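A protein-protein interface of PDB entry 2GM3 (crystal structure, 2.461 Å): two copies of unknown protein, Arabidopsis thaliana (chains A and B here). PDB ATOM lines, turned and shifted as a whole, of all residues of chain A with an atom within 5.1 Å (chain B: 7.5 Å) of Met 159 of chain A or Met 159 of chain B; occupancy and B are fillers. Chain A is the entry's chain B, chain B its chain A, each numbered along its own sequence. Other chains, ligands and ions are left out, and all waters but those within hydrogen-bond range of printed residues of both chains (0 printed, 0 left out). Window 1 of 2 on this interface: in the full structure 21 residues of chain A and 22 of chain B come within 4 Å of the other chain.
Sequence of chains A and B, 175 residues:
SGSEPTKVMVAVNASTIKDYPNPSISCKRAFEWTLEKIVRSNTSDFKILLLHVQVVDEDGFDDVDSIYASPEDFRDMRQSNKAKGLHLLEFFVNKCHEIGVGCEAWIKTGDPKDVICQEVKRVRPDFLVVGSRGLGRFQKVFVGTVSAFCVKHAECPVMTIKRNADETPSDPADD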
ATOM      1  N   TRP A  33      11.704  30.898  -2.920  1.00  0.00           N
ATOM      2  CA  TRP A  33      12.396  31.530  -4.016  1.00  0.00           C
ATOM      3  C   TRP A  33      11.373  31.951  -5.075  1.00  0.00           C
ATOM      4  O   TRP A  33      11.423  33.074  -5.579  1.00  0.00           O
ATOM      5  CB  TRP A  33      13.487  30.648  -4.609  1.00  0.00           C
ATOM      6  CG  TRP A  33      14.127  31.331  -5.759  1.00  0.00           C
ATOM      7  CD1 TRP A  33      15.216  32.166  -5.725  1.00  0.00           C
ATOM      8  CD2 TRP A  33      13.683  31.294  -7.116  1.00  0.00           C
ATOM      9  NE1 TRP A  33      15.491  32.616  -6.989  1.00  0.00           N
ATOM     10  CE2 TRP A  33      14.563  32.102  -7.862  1.00  0.00           C
ATOM     11  CE3 TRP A  33      12.654  30.616  -7.780  1.00  0.00           C
ATOM     12  CZ2 TRP A  33      14.442  32.265  -9.249  1.00  0.00           C
ATOM     13  CZ3 TRP A  33      12.517  30.777  -9.166  1.00  0.00           C
ATOM     14  CH2 TRP A  33      13.410  31.599  -9.878  1.00  0.00           C
ATOM     15  N   ILE A  38       9.903  35.170  -8.644  1.00  0.00           N
ATOM     16  CA  ILE A  38       8.953  35.014  -9.742  1.00  0.00           C
ATOM     17  C   ILE A  38       7.679  35.809  -9.484  1.00  0.00           C
ATOM     18  O   ILE A  38       7.257  36.610 -10.315  1.00  0.00           O
ATOM     19  CB  ILE A  38       8.580  33.516  -9.969  1.00  0.00           C
ATOM     20  CG1 ILE A  38       9.836  32.672 -10.301  1.00  0.00           C
ATOM     21  CG2 ILE A  38       7.406  33.374 -10.992  1.00  0.00           C
ATOM     22  CD1 ILE A  38      10.549  33.062 -11.572  1.00  0.00           C
ATOM     23  N   PHE A 127       3.522  25.834 -15.015  1.00  0.00           N
ATOM     24  CA  PHE A 127       4.768  25.127 -14.721  1.00  0.00           C
ATOM     25  C   PHE A 127       4.800  24.542 -13.332  1.00  0.00           C
ATOM     26  O   PHE A 127       3.942  24.821 -12.506  1.00  0.00           O
ATOM     27  CB  PHE A 127       6.038  25.961 -15.006  1.00  0.00           C
ATOM     28  CG  PHE A 127       6.241  27.121 -14.067  1.00  0.00           C
ATOM     29  CD1 PHE A 127       7.122  27.016 -12.995  1.00  0.00           C
ATOM     30  CD2 PHE A 127       5.571  28.320 -14.265  1.00  0.00           C
ATOM     31  CE1 PHE A 127       7.347  28.082 -12.150  1.00  0.00           C
ATOM     32  CE2 PHE A 127       5.789  29.397 -13.415  1.00  0.00           C
ATOM     33  CZ  PHE A 127       6.667  29.281 -12.347  1.00  0.00           C
ATOM     34  N   LEU A 128       5.811  23.708 -13.116  1.00  0.00           N
ATOM     35  CA  LEU A 128       6.010  22.901 -11.936  1.00  0.00           C
ATOM     36  C   LEU A 128       7.266  23.361 -11.245  1.00  0.00           C
ATOM     37  O   LEU A 128       8.335  23.452 -11.859  1.00  0.00           O
ATOM     38  CB  LEU A 128       6.212  21.430 -12.336  1.00  0.00           C
ATOM     39  CG  LEU A 128       6.582  20.431 -11.225  1.00  0.00           C
ATOM     40  CD1 LEU A 128       5.511  20.432 -10.112  1.00  0.00           C
ATOM     41  CD2 LEU A 128       6.824  19.012 -11.733  1.00  0.00           C
ATOM     42  N   VAL A 129       7.152  23.606  -9.954  1.00  0.00           N
ATOM     43  CA  VAL A 129       8.301  23.921  -9.143  1.00  0.00           C
ATOM     44  C   VAL A 129       8.579  22.763  -8.223  1.00  0.00           C
ATOM     45  O   VAL A 129       7.689  22.279  -7.537  1.00  0.00           O
ATOM     46  CB  VAL A 129       8.101  25.222  -8.321  1.00  0.00           C
ATOM     47  CG1 VAL A 129       9.221  25.397  -7.295  1.00  0.00           C
ATOM     48  CG2 VAL A 129       8.023  26.405  -9.251  1.00  0.00           C
ATOM     49  N   VAL A 130       9.807  22.275  -8.260  1.00  0.00           N
ATOM     50  CA  VAL A 130      10.242  21.235  -7.343  1.00  0.00           C
ATOM     51  C   VAL A 130      11.546  21.694  -6.769  1.00  0.00           C
ATOM     52  O   VAL A 130      12.363  22.331  -7.458  1.00  0.00           O
ATOM     53  CB  VAL A 130      10.407  19.868  -8.038  1.00  0.00           C
ATOM     54  CG1 VAL A 130       9.060  19.462  -8.635  1.00  0.00           C
ATOM     55  CG2 VAL A 130      11.538  19.877  -9.143  1.00  0.00           C
ATOM     56  N   PRO A 157       6.598  22.901 -18.415  1.00  0.00           N
ATOM     57  CA  PRO A 157       7.903  23.354 -17.909  1.00  0.00           C
ATOM     58  C   PRO A 157       8.129  23.089 -16.415  1.00  0.00           C
ATOM     59  O   PRO A 157       7.202  23.093 -15.611  1.00  0.00           O
ATOM     60  CB  PRO A 157       7.911  24.853 -18.235  1.00  0.00           C
ATOM     61  CG  PRO A 157       6.963  24.978 -19.420  1.00  0.00           C
ATOM     62  CD  PRO A 157       5.928  23.908 -19.265  1.00  0.00           C
ATOM     63  N   VAL A 158       9.387  22.845 -16.080  1.00  0.00           N
ATOM     64  CA  VAL A 158       9.795  22.521 -14.738  1.00  0.00           C
ATOM     65  C   VAL A 158      10.863  23.483 -14.238  1.00  0.00           C
ATOM     66  O   VAL A 158      11.889  23.726 -14.885  1.00  0.00           O
ATOM     67  CB  VAL A 158      10.341  21.091 -14.682  1.00  0.00           C
ATOM     68  CG1 VAL A 158      10.801  20.777 -13.285  1.00  0.00           C
ATOM     69  CG2 VAL A 158       9.248  20.094 -15.112  1.00  0.00           C
ATOM     70  N   MET A 159      10.638  24.030 -13.063  1.00  0.00           N
ATOM     71  CA  MET A 159      11.647  24.844 -12.432  1.00  0.00           C
ATOM     72  C   MET A 159      12.234  24.016 -11.287  1.00  0.00           C
ATOM     73  O   MET A 159      11.498  23.609 -10.343  1.00  0.00           O
ATOM     74  CB  MET A 159      10.982  26.107 -11.913  1.00  0.00           C
ATOM     75  CG  MET A 159      11.825  26.965 -10.977  1.00  0.00           C
ATOM     76  SD  MET A 159      12.971  28.029 -12.022  1.00  0.00           S
ATOM     77  CE  MET A 159      11.884  29.555 -12.100  1.00  0.00           C
ATOM     78  N   THR A 160      13.527  23.749 -11.359  1.00  0.00           N
ATOM     79  CA  THR A 160      14.190  22.978 -10.331  1.00  0.00           C
ATOM     80  C   THR A 160      15.026  23.910  -9.497  1.00  0.00           C
ATOM     81  O   THR A 160      15.842  24.652 -10.026  1.00  0.00           O
ATOM     82  CB  THR A 160      15.112  21.939 -10.925  1.00  0.00           C
ATOM     83  OG1 THR A 160      14.418  21.274 -11.976  1.00  0.00           O
ATOM     84  CG2 THR A 160      15.507  20.935  -9.862  1.00  0.00           C
ATOM     85  N   ILE A 161      14.819  23.870  -8.194  1.00  0.00           N
ATOM     86  CA  ILE A 161      15.494  24.771  -7.303  1.00  0.00           C
ATOM     87  C   ILE A 161      16.231  23.963  -6.278  1.00  0.00           C
ATOM     88  O   ILE A 161      15.630  23.181  -5.550  1.00  0.00           O
ATOM     89  CB  ILE A 161      14.516  25.693  -6.602  1.00  0.00           C
ATOM     90  CG1 ILE A 161      13.799  26.523  -7.655  1.00  0.00           C
ATOM     91  CG2 ILE A 161      15.257  26.556  -5.629  1.00  0.00           C
ATOM     92  CD1 ILE A 161      12.505  27.023  -7.239  1.00  0.00           C
ATOM     93  N   VAL B   8      16.845  37.033 -15.204  1.00  0.00           N
ATOM     94  CA  VAL B   8      16.569  35.794 -15.862  1.00  0.00           C
ATOM     95  C   VAL B   8      17.639  35.555 -16.929  1.00  0.00           C
ATOM     96  O   VAL B   8      17.652  36.242 -17.961  1.00  0.00           O
ATOM     97  CB  VAL B   8      15.202  35.881 -16.535  1.00  0.00           C
ATOM     98  CG1 VAL B   8      14.793  34.517 -17.112  1.00  0.00           C
ATOM     99  CG2 VAL B   8      14.171  36.397 -15.555  1.00  0.00           C
ATOM    100  N   MET B   9      18.512  34.569 -16.694  1.00  0.00           N
ATOM    101  CA  MET B   9      19.498  34.179 -17.714  1.00  0.00           C
ATOM    102  C   MET B   9      18.870  33.202 -18.690  1.00  0.00           C
ATOM    103  O   MET B   9      18.272  32.218 -18.261  1.00  0.00           O
ATOM    104  CB  MET B   9      20.722  33.540 -17.082  1.00  0.00           C
ATOM    105  CG  MET B   9      21.837  33.353 -18.126  1.00  0.00           C
ATOM    106  SD  MET B   9      23.536  32.944 -17.337  1.00  0.00           S
ATOM    107  CE  MET B   9      23.716  31.323 -18.083  1.00  0.00           C
ATOM    108  N   ALA B  30      11.544  28.472 -25.328  1.00  0.00           N
ATOM    109  CA  ALA B  30      11.914  28.777 -23.955  1.00  0.00           C
ATOM    110  C   ALA B  30      11.830  30.278 -23.635  1.00  0.00           C
ATOM    111  O   ALA B  30      11.283  30.671 -22.608  1.00  0.00           O
ATOM    112  CB  ALA B  30      13.295  28.275 -23.688  1.00  0.00           C
ATOM    113  N   TRP B  33       8.075  31.603 -24.051  1.00  0.00           N
ATOM    114  CA  TRP B  33       7.283  31.122 -22.968  1.00  0.00           C
ATOM    115  C   TRP B  33       7.567  31.940 -21.714  1.00  0.00           C
ATOM    116  O   TRP B  33       6.626  32.325 -21.011  1.00  0.00           O
ATOM    117  CB  TRP B  33       7.607  29.661 -22.707  1.00  0.00           C
ATOM    118  CG  TRP B  33       6.745  29.020 -21.699  1.00  0.00           C
ATOM    119  CD1 TRP B  33       5.591  28.322 -21.936  1.00  0.00           C
ATOM    120  CD2 TRP B  33       6.950  28.988 -20.291  1.00  0.00           C
ATOM    121  NE1 TRP B  33       5.079  27.865 -20.775  1.00  0.00           N
ATOM    122  CE2 TRP B  33       5.887  28.251 -19.738  1.00  0.00           C
ATOM    123  CE3 TRP B  33       7.922  29.521 -19.435  1.00  0.00           C
ATOM    124  CZ2 TRP B  33       5.754  28.037 -18.365  1.00  0.00           C
ATOM    125  CZ3 TRP B  33       7.797  29.295 -18.066  1.00  0.00           C
ATOM    126  CH2 TRP B  33       6.724  28.545 -17.551  1.00  0.00           C
ATOM    127  N   THR B  34       8.848  32.174 -21.431  1.00  0.00           N
ATOM    128  CA  THR B  34       9.231  32.975 -20.293  1.00  0.00           C
ATOM    129  C   THR B  34       8.630  34.362 -20.346  1.00  0.00           C
ATOM    130  O   THR B  34       8.156  34.822 -19.331  1.00  0.00           O
ATOM    131  CB  THR B  34      10.772  33.069 -20.115  1.00  0.00           C
ATOM    132  OG1 THR B  34      11.317  31.750 -20.041  1.00  0.00           O
ATOM    133  CG2 THR B  34      11.115  33.791 -18.824  1.00  0.00           C
ATOM    134  N   ILE B  38       6.002  34.237 -17.494  1.00  0.00           N
ATOM    135  CA  ILE B  38       6.715  34.769 -16.317  1.00  0.00           C
ATOM    136  C   ILE B  38       6.812  36.299 -16.286  1.00  0.00           C
ATOM    137  O   ILE B  38       6.414  36.918 -15.312  1.00  0.00           O
ATOM    138  CB  ILE B  38       8.128  34.109 -16.117  1.00  0.00           C
ATOM    139  CG1 ILE B  38       8.030  32.571 -16.133  1.00  0.00           C
ATOM    140  CG2 ILE B  38       8.874  34.655 -14.856  1.00  0.00           C
ATOM    141  CD1 ILE B  38       7.939  31.932 -14.796  1.00  0.00           C
ATOM    142  N   ASP B 126      19.022  35.270 -11.099  1.00  0.00           N
ATOM    143  CA  ASP B 126      18.151  34.689 -10.131  1.00  0.00           C
ATOM    144  C   ASP B 126      17.763  33.293 -10.608  1.00  0.00           C
ATOM    145  O   ASP B 126      17.675  32.379  -9.802  1.00  0.00           O
ATOM    146  CB  ASP B 126      16.953  35.575  -9.909  1.00  0.00           C
ATOM    147  CG  ASP B 126      17.329  36.899  -9.282  1.00  0.00           C
ATOM    148  OD1 ASP B 126      17.815  36.924  -8.133  1.00  0.00           O
ATOM    149  OD2 ASP B 126      17.143  37.931  -9.948  1.00  0.00           O
ATOM    150  N   PHE B 127      17.543  33.142 -11.914  1.00  0.00           N
ATOM    151  CA  PHE B 127      17.404  31.848 -12.506  1.00  0.00           C
ATOM    152  C   PHE B 127      17.879  31.725 -13.937  1.00  0.00           C
ATOM    153  O   PHE B 127      18.070  32.725 -14.629  1.00  0.00           O
ATOM    154  CB  PHE B 127      15.993  31.281 -12.327  1.00  0.00           C
ATOM    155  CG  PHE B 127      14.900  31.983 -13.095  1.00  0.00           C
ATOM    156  CD1 PHE B 127      14.302  31.355 -14.171  1.00  0.00           C
ATOM    157  CD2 PHE B 127      14.398  33.214 -12.672  1.00  0.00           C
ATOM    158  CE1 PHE B 127      13.239  31.967 -14.864  1.00  0.00           C
ATOM    159  CE2 PHE B 127      13.367  33.826 -13.339  1.00  0.00           C
ATOM    160  CZ  PHE B 127      12.776  33.208 -14.440  1.00  0.00           C
ATOM    161  N   LEU B 128      18.027  30.472 -14.372  1.00  0.00           N
ATOM    162  CA  LEU B 128      18.462  30.117 -15.720  1.00  0.00           C
ATOM    163  C   LEU B 128      17.307  29.473 -16.475  1.00  0.00           C
ATOM    164  O   LEU B 128      16.675  28.536 -15.978  1.00  0.00           O
ATOM    165  CB  LEU B 128      19.630  29.115 -15.595  1.00  0.00           C
ATOM    166  CG  LEU B 128      20.184  28.414 -16.827  1.00  0.00           C
ATOM    167  CD1 LEU B 128      20.633  29.460 -17.866  1.00  0.00           C
ATOM    168  CD2 LEU B 128      21.306  27.501 -16.485  1.00  0.00           C
ATOM    169  N   VAL B 129      17.021  29.979 -17.660  1.00  0.00           N
ATOM    170  CA  VAL B 129      16.076  29.339 -18.562  1.00  0.00           C
ATOM    171  C   VAL B 129      16.839  28.657 -19.712  1.00  0.00           C
ATOM    172  O   VAL B 129      17.664  29.285 -20.386  1.00  0.00           O
ATOM    173  CB  VAL B 129      15.100  30.354 -19.163  1.00  0.00           C
ATOM    174  CG1 VAL B 129      14.149  29.669 -20.104  1.00  0.00           C
ATOM    175  CG2 VAL B 129      14.323  31.104 -18.084  1.00  0.00           C
ATOM    176  N   VAL B 130      16.569  27.373 -19.908  1.00  0.00           N
ATOM    177  CA  VAL B 130      17.091  26.647 -21.025  1.00  0.00           C
ATOM    178  C   VAL B 130      15.917  25.971 -21.668  1.00  0.00           C
ATOM    179  O   VAL B 130      14.973  25.546 -20.980  1.00  0.00           O
ATOM    180  CB  VAL B 130      18.173  25.563 -20.606  1.00  0.00           C
ATOM    181  CG1 VAL B 130      19.452  26.252 -20.100  1.00  0.00           C
ATOM    182  CG2 VAL B 130      17.632  24.627 -19.528  1.00  0.00           C
ATOM    183  N   GLY B 131      15.964  25.889 -22.989  1.00  0.00           N
ATOM    184  CA  GLY B 131      15.074  25.044 -23.735  1.00  0.00           C
ATOM    185  C   GLY B 131      15.559  23.623 -23.518  1.00  0.00           C
ATOM    186  O   GLY B 131      16.585  23.414 -22.872  1.00  0.00           O
ATOM    187  N   SER B 132      14.817  22.648 -24.040  1.00  0.00           N
ATOM    188  CA  SER B 132      15.204  21.268 -23.932  1.00  0.00           C
ATOM    189  C   SER B 132      14.541  20.489 -25.044  1.00  0.00           C
ATOM    190  O   SER B 132      13.376  20.710 -25.346  1.00  0.00           O
ATOM    191  CB  SER B 132      14.785  20.707 -22.578  1.00  0.00           C
ATOM    192  OG  SER B 132      14.893  19.287 -22.587  1.00  0.00           O
ATOM    193  N   SER B 147      20.656  20.951 -21.389  1.00  0.00           N
ATOM    194  CA  SER B 147      19.646  21.275 -20.382  1.00  0.00           C
ATOM    195  C   SER B 147      19.770  20.391 -19.150  1.00  0.00           C
ATOM    196  O   SER B 147      19.633  20.889 -18.048  1.00  0.00           O
ATOM    197  CB  SER B 147      18.216  21.231 -20.941  1.00  0.00           C
ATOM    198  OG  SER B 147      17.818  19.904 -21.329  1.00  0.00           O
ATOM    199  N   VAL B 151      20.525  21.724 -15.177  1.00  0.00           N
ATOM    200  CA  VAL B 151      19.606  21.416 -14.098  1.00  0.00           C
ATOM    201  C   VAL B 151      20.377  20.779 -12.958  1.00  0.00           C
ATOM    202  O   VAL B 151      20.142  21.085 -11.782  1.00  0.00           O
ATOM    203  CB  VAL B 151      18.519  20.425 -14.601  1.00  0.00           C
ATOM    204  CG1 VAL B 151      17.782  19.751 -13.438  1.00  0.00           C
ATOM    205  CG2 VAL B 151      17.575  21.143 -15.561  1.00  0.00           C
ATOM    206  N   CYS B 156      21.984  28.081  -9.596  1.00  0.00           N
ATOM    207  CA  CYS B 156      20.797  28.881  -9.461  1.00  0.00           C
ATOM    208  C   CYS B 156      19.628  27.991  -9.894  1.00  0.00           C
ATOM    209  O   CYS B 156      19.851  26.941 -10.487  1.00  0.00           O
ATOM    210  CB  CYS B 156      20.891  30.101 -10.377  1.00  0.00           C
ATOM    211  SG  CYS B 156      20.835  29.632 -12.063  1.00  0.00           S
ATOM    212  N   PRO B 157      18.386  28.404  -9.601  1.00  0.00           N
ATOM    213  CA  PRO B 157      17.197  27.744 -10.166  1.00  0.00           C
ATOM    214  C   PRO B 157      17.254  27.619 -11.680  1.00  0.00           C
ATOM    215  O   PRO B 157      17.711  28.535 -12.371  1.00  0.00           O
ATOM    216  CB  PRO B 157      16.063  28.694  -9.791  1.00  0.00           C
ATOM    217  CG  PRO B 157      16.539  29.275  -8.448  1.00  0.00           C
ATOM    218  CD  PRO B 157      18.028  29.482  -8.657  1.00  0.00           C
ATOM    219  N   VAL B 158      16.799  26.485 -12.184  1.00  0.00           N
ATOM    220  CA  VAL B 158      16.797  26.221 -13.601  1.00  0.00           C
ATOM    221  C   VAL B 158      15.372  25.908 -14.051  1.00  0.00           C
ATOM    222  O   VAL B 158      14.700  25.099 -13.448  1.00  0.00           O
ATOM    223  CB  VAL B 158      17.771  25.033 -13.994  1.00  0.00           C
ATOM    224  CG1 VAL B 158      17.855  24.912 -15.492  1.00  0.00           C
ATOM    225  CG2 VAL B 158      19.179  25.258 -13.457  1.00  0.00           C
ATOM    226  N   MET B 159      14.936  26.585 -15.092  1.00  0.00           N
ATOM    227  CA  MET B 159      13.656  26.393 -15.681  1.00  0.00           C
ATOM    228  C   MET B 159      13.962  25.710 -16.993  1.00  0.00           C
ATOM    229  O   MET B 159      14.672  26.283 -17.828  1.00  0.00           O
ATOM    230  CB  MET B 159      13.046  27.764 -15.975  1.00  0.00           C
ATOM    231  CG  MET B 159      11.744  27.682 -16.744  1.00  0.00           C
ATOM    232  SD  MET B 159      10.343  26.981 -15.593  1.00  0.00           S
ATOM    233  CE  MET B 159       9.895  28.569 -14.822  1.00  0.00           C
ATOM    234  N   THR B 160      13.453  24.493 -17.179  1.00  0.00           N
ATOM    235  CA  THR B 160      13.613  23.786 -18.440  1.00  0.00           C
ATOM    236  C   THR B 160      12.266  23.772 -19.141  1.00  0.00           C
ATOM    237  O   THR B 160      11.274  23.297 -18.577  1.00  0.00           O
ATOM    238  CB  THR B 160      14.098  22.310 -18.289  1.00  0.00           C
ATOM    239  OG1 THR B 160      13.239  21.633 -17.392  1.00  0.00           O
ATOM    240  CG2 THR B 160      15.429  22.247 -17.686  1.00  0.00           C
ATOM    241  N   ILE B 161      12.249  24.306 -20.369  1.00  0.00           N
ATOM    242  CA  ILE B 161      11.053  24.390 -21.187  1.00  0.00           C
ATOM    243  C   ILE B 161      11.264  23.583 -22.434  1.00  0.00           C
ATOM    244  O   ILE B 161      12.238  23.797 -23.132  1.00  0.00           O
ATOM    245  CB  ILE B 161      10.744  25.877 -21.565  1.00  0.00           C
ATOM    246  CG1 ILE B 161      10.579  26.714 -20.284  1.00  0.00           C
ATOM    247  CG2 ILE B 161       9.483  25.987 -22.471  1.00  0.00           C
ATOM    248  CD1 ILE B 161      11.134  28.047 -20.349  1.00  0.00           C
ATOM    249  N   LYS B 162      10.352  22.647 -22.686  1.00  0.00           N
ATOM    250  CA  LYS B 162      10.363  21.779 -23.846  1.00  0.00           C
ATOM    251  C   LYS B 162       9.492  22.388 -24.904  1.00  0.00           C
ATOM    252  O   LYS B 162       8.685  23.247 -24.607  1.00  0.00           O
ATOM    253  CB  LYS B 162       9.816  20.395 -23.528  1.00  0.00           C
ATOM    254  CG  LYS B 162      10.764  19.554 -22.685  1.00  0.00           C
ATOM    255  CD  LYS B 162      10.005  18.367 -22.060  1.00  0.00           C
ATOM    256  CE  LYS B 162      10.807  17.696 -20.941  1.00  0.00           C
ATOM    257  NZ  LYS B 162       9.877  17.258 -19.794  1.00  0.00           N
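Trp 33 of chain A touches Phe 127 of chain B, and with the chains exchanged Phe 127 of chain A touches Trp 33 of chain B. Pro 157 of chain A touches Thr 160 of chain B, and with the chains exchanged Thr 160 of chain A touches Pro 157 of chain B. Val 158 of chain A touches Thr 160 of chain B, and with the chains exchanged Thr 160 of chain A touches Val 158 of chain B. Met 159 of chain A touches Pro 157 of chain B, but with the chains exchanged Pro 157 of chain A does not touch Met 159 of chain B (4.2 Å).
The backbone carbonyl oxygen (O) of Val 158 of chain B lies within hydrogen-bond range of the backbone NH (N) of Thr 160 of chain A, 2.7 Å away. The backbone NH (N) of Thr 160 of chain B is in hydrogen-bond range of the backbone carbonyl oxygen (O) of Val 158 of chain A, 2.9 Å away. The backbone carbonyl oxygen of Val 158 of chain A lies close to the backbone carbonyl oxygen of Val 158 of chain B (3.4 Å). The side-chain sulfur (SD) of Met 159 of chain B sits close to the backbone carbonyl oxygen (O) of Val 158 of chain A (3.7 Å). SD of Met 159 of chain A sits close to O of Val 158 of chain B (3.7 Å).
The backbone NH of Leu 128 of chain B is in hydrogen-bond range of the backbone carbonyl oxygen of Pro 157 of chain B, 2.8 Å away. The backbone carbonyl oxygen of Leu 128 of chain B lies within hydrogen-bond range of the backbone NH of Met 159 of chain B (2.8 Å). N of Val 130 of chain B is in hydrogen-bond range of O of Met 159 of chain B (3.0 Å). The backbone carbonyl oxygen of Val 130 of chain B lies within hydrogen-bond range of the backbone NH of Ile 161 of chain B (3.1 Å). O of Pro 157 of chain A lies within hydrogen-bond range of N of Leu 128 of chain A (2.9 Å). The backbone NH (N) of Val 130 of chain A is in hydrogen-bond range of the backbone carbonyl oxygen (O) of Met 159 of chain A (3.0 Å).
Printed residues of chain B that touch a printed residue of chain A: Trp 33, Ile 38, Asp 126, Phe 127, Val 151, Pro 157, Val 158, Met 159, Thr 160 and Ile 161. Hydrophobic or aromatic side chains of chain B that line the printed part of chain A: Trp 33, Ile 38, Phe 127, Val 151, Pro 157, Met 159 and Ile 161. Along chain B the printed residues that touch a printed residue of chain A span positions 33 to 161. Printed residues of chain A that touch a printed residue of chain B: Trp 33, Ile 38, Phe 127, Pro 157, Val 158, Met 159, Thr 160 and Ile 161. Hydrophobic or aromatic side chains of chain A within 4 Å of the printed part of chain B: Trp 33, Ile 38, Phe 127, Pro 157, Met 159 and Ile 161. Among the printed residues, no Asp or Glu carboxylate lies within 4 Å of a Lys or Arg side-chain nitrogen of the other chain.
Among the printed residues, merely in contact across the chains: Trp 33 of chain A with Asp 126 of chain B (3.3 Å), Trp 33 of chain A with Phe 127 of chain B (3.4 Å), Thr 160 of chain A with Pro 157 of chain B (3.4 Å), Ile 38 of chain A with Phe 127 of chain B (3.4 Å), Pro 157 of chain A with Thr 160 of chain B (3.4 Å), Pro 157 of chain A with Trp 33 of chain B (3.5 Å), Phe 127 of chain A with Trp 33 of chain B (3.5 Å), Trp 33 of chain A with Pro 157 of chain B (3.5 Å), Met 159 of chain A with Met 159 of chain B (3.5 Å), Phe 127 of chain A with Ile 38 of chain B (3.6 Å), Met 159 of chain A with Phe 127 of chain B (3.7 Å), Phe 127 of chain A with Met 159 of chain B (3.7 Å), Ile 161 of chain A with Pro 157 of chain B (3.8 Å), Pro 157 of chain A with Ile 161 of chain B (3.8 Å), Met 159 of chain A with Pro 157 of chain B (3.9 Å) and Thr 160 of chain A with Val 151 of chain B (3.97 Å).
Printed residues of chain B within 4 Å of Ile 38 of chain A: Phe 127. Of the printed residues of chain B, Phe 127 of chain A touches Trp 33, Ile 38 and Met 159. Printed residues of chain B within 4 Å of Met 159 of chain A: Phe 127 (3.7 Å), Pro 157 (3.9 Å), Val 158 (3.2 Å) and Met 159 (3.5 Å). Of the printed residues of chain A, Pro 157 of chain B touches Trp 33 (3.5 Å), Met 159 (3.9 Å), Thr 160 (3.4 Å) and Ile 161 (3.8 Å).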
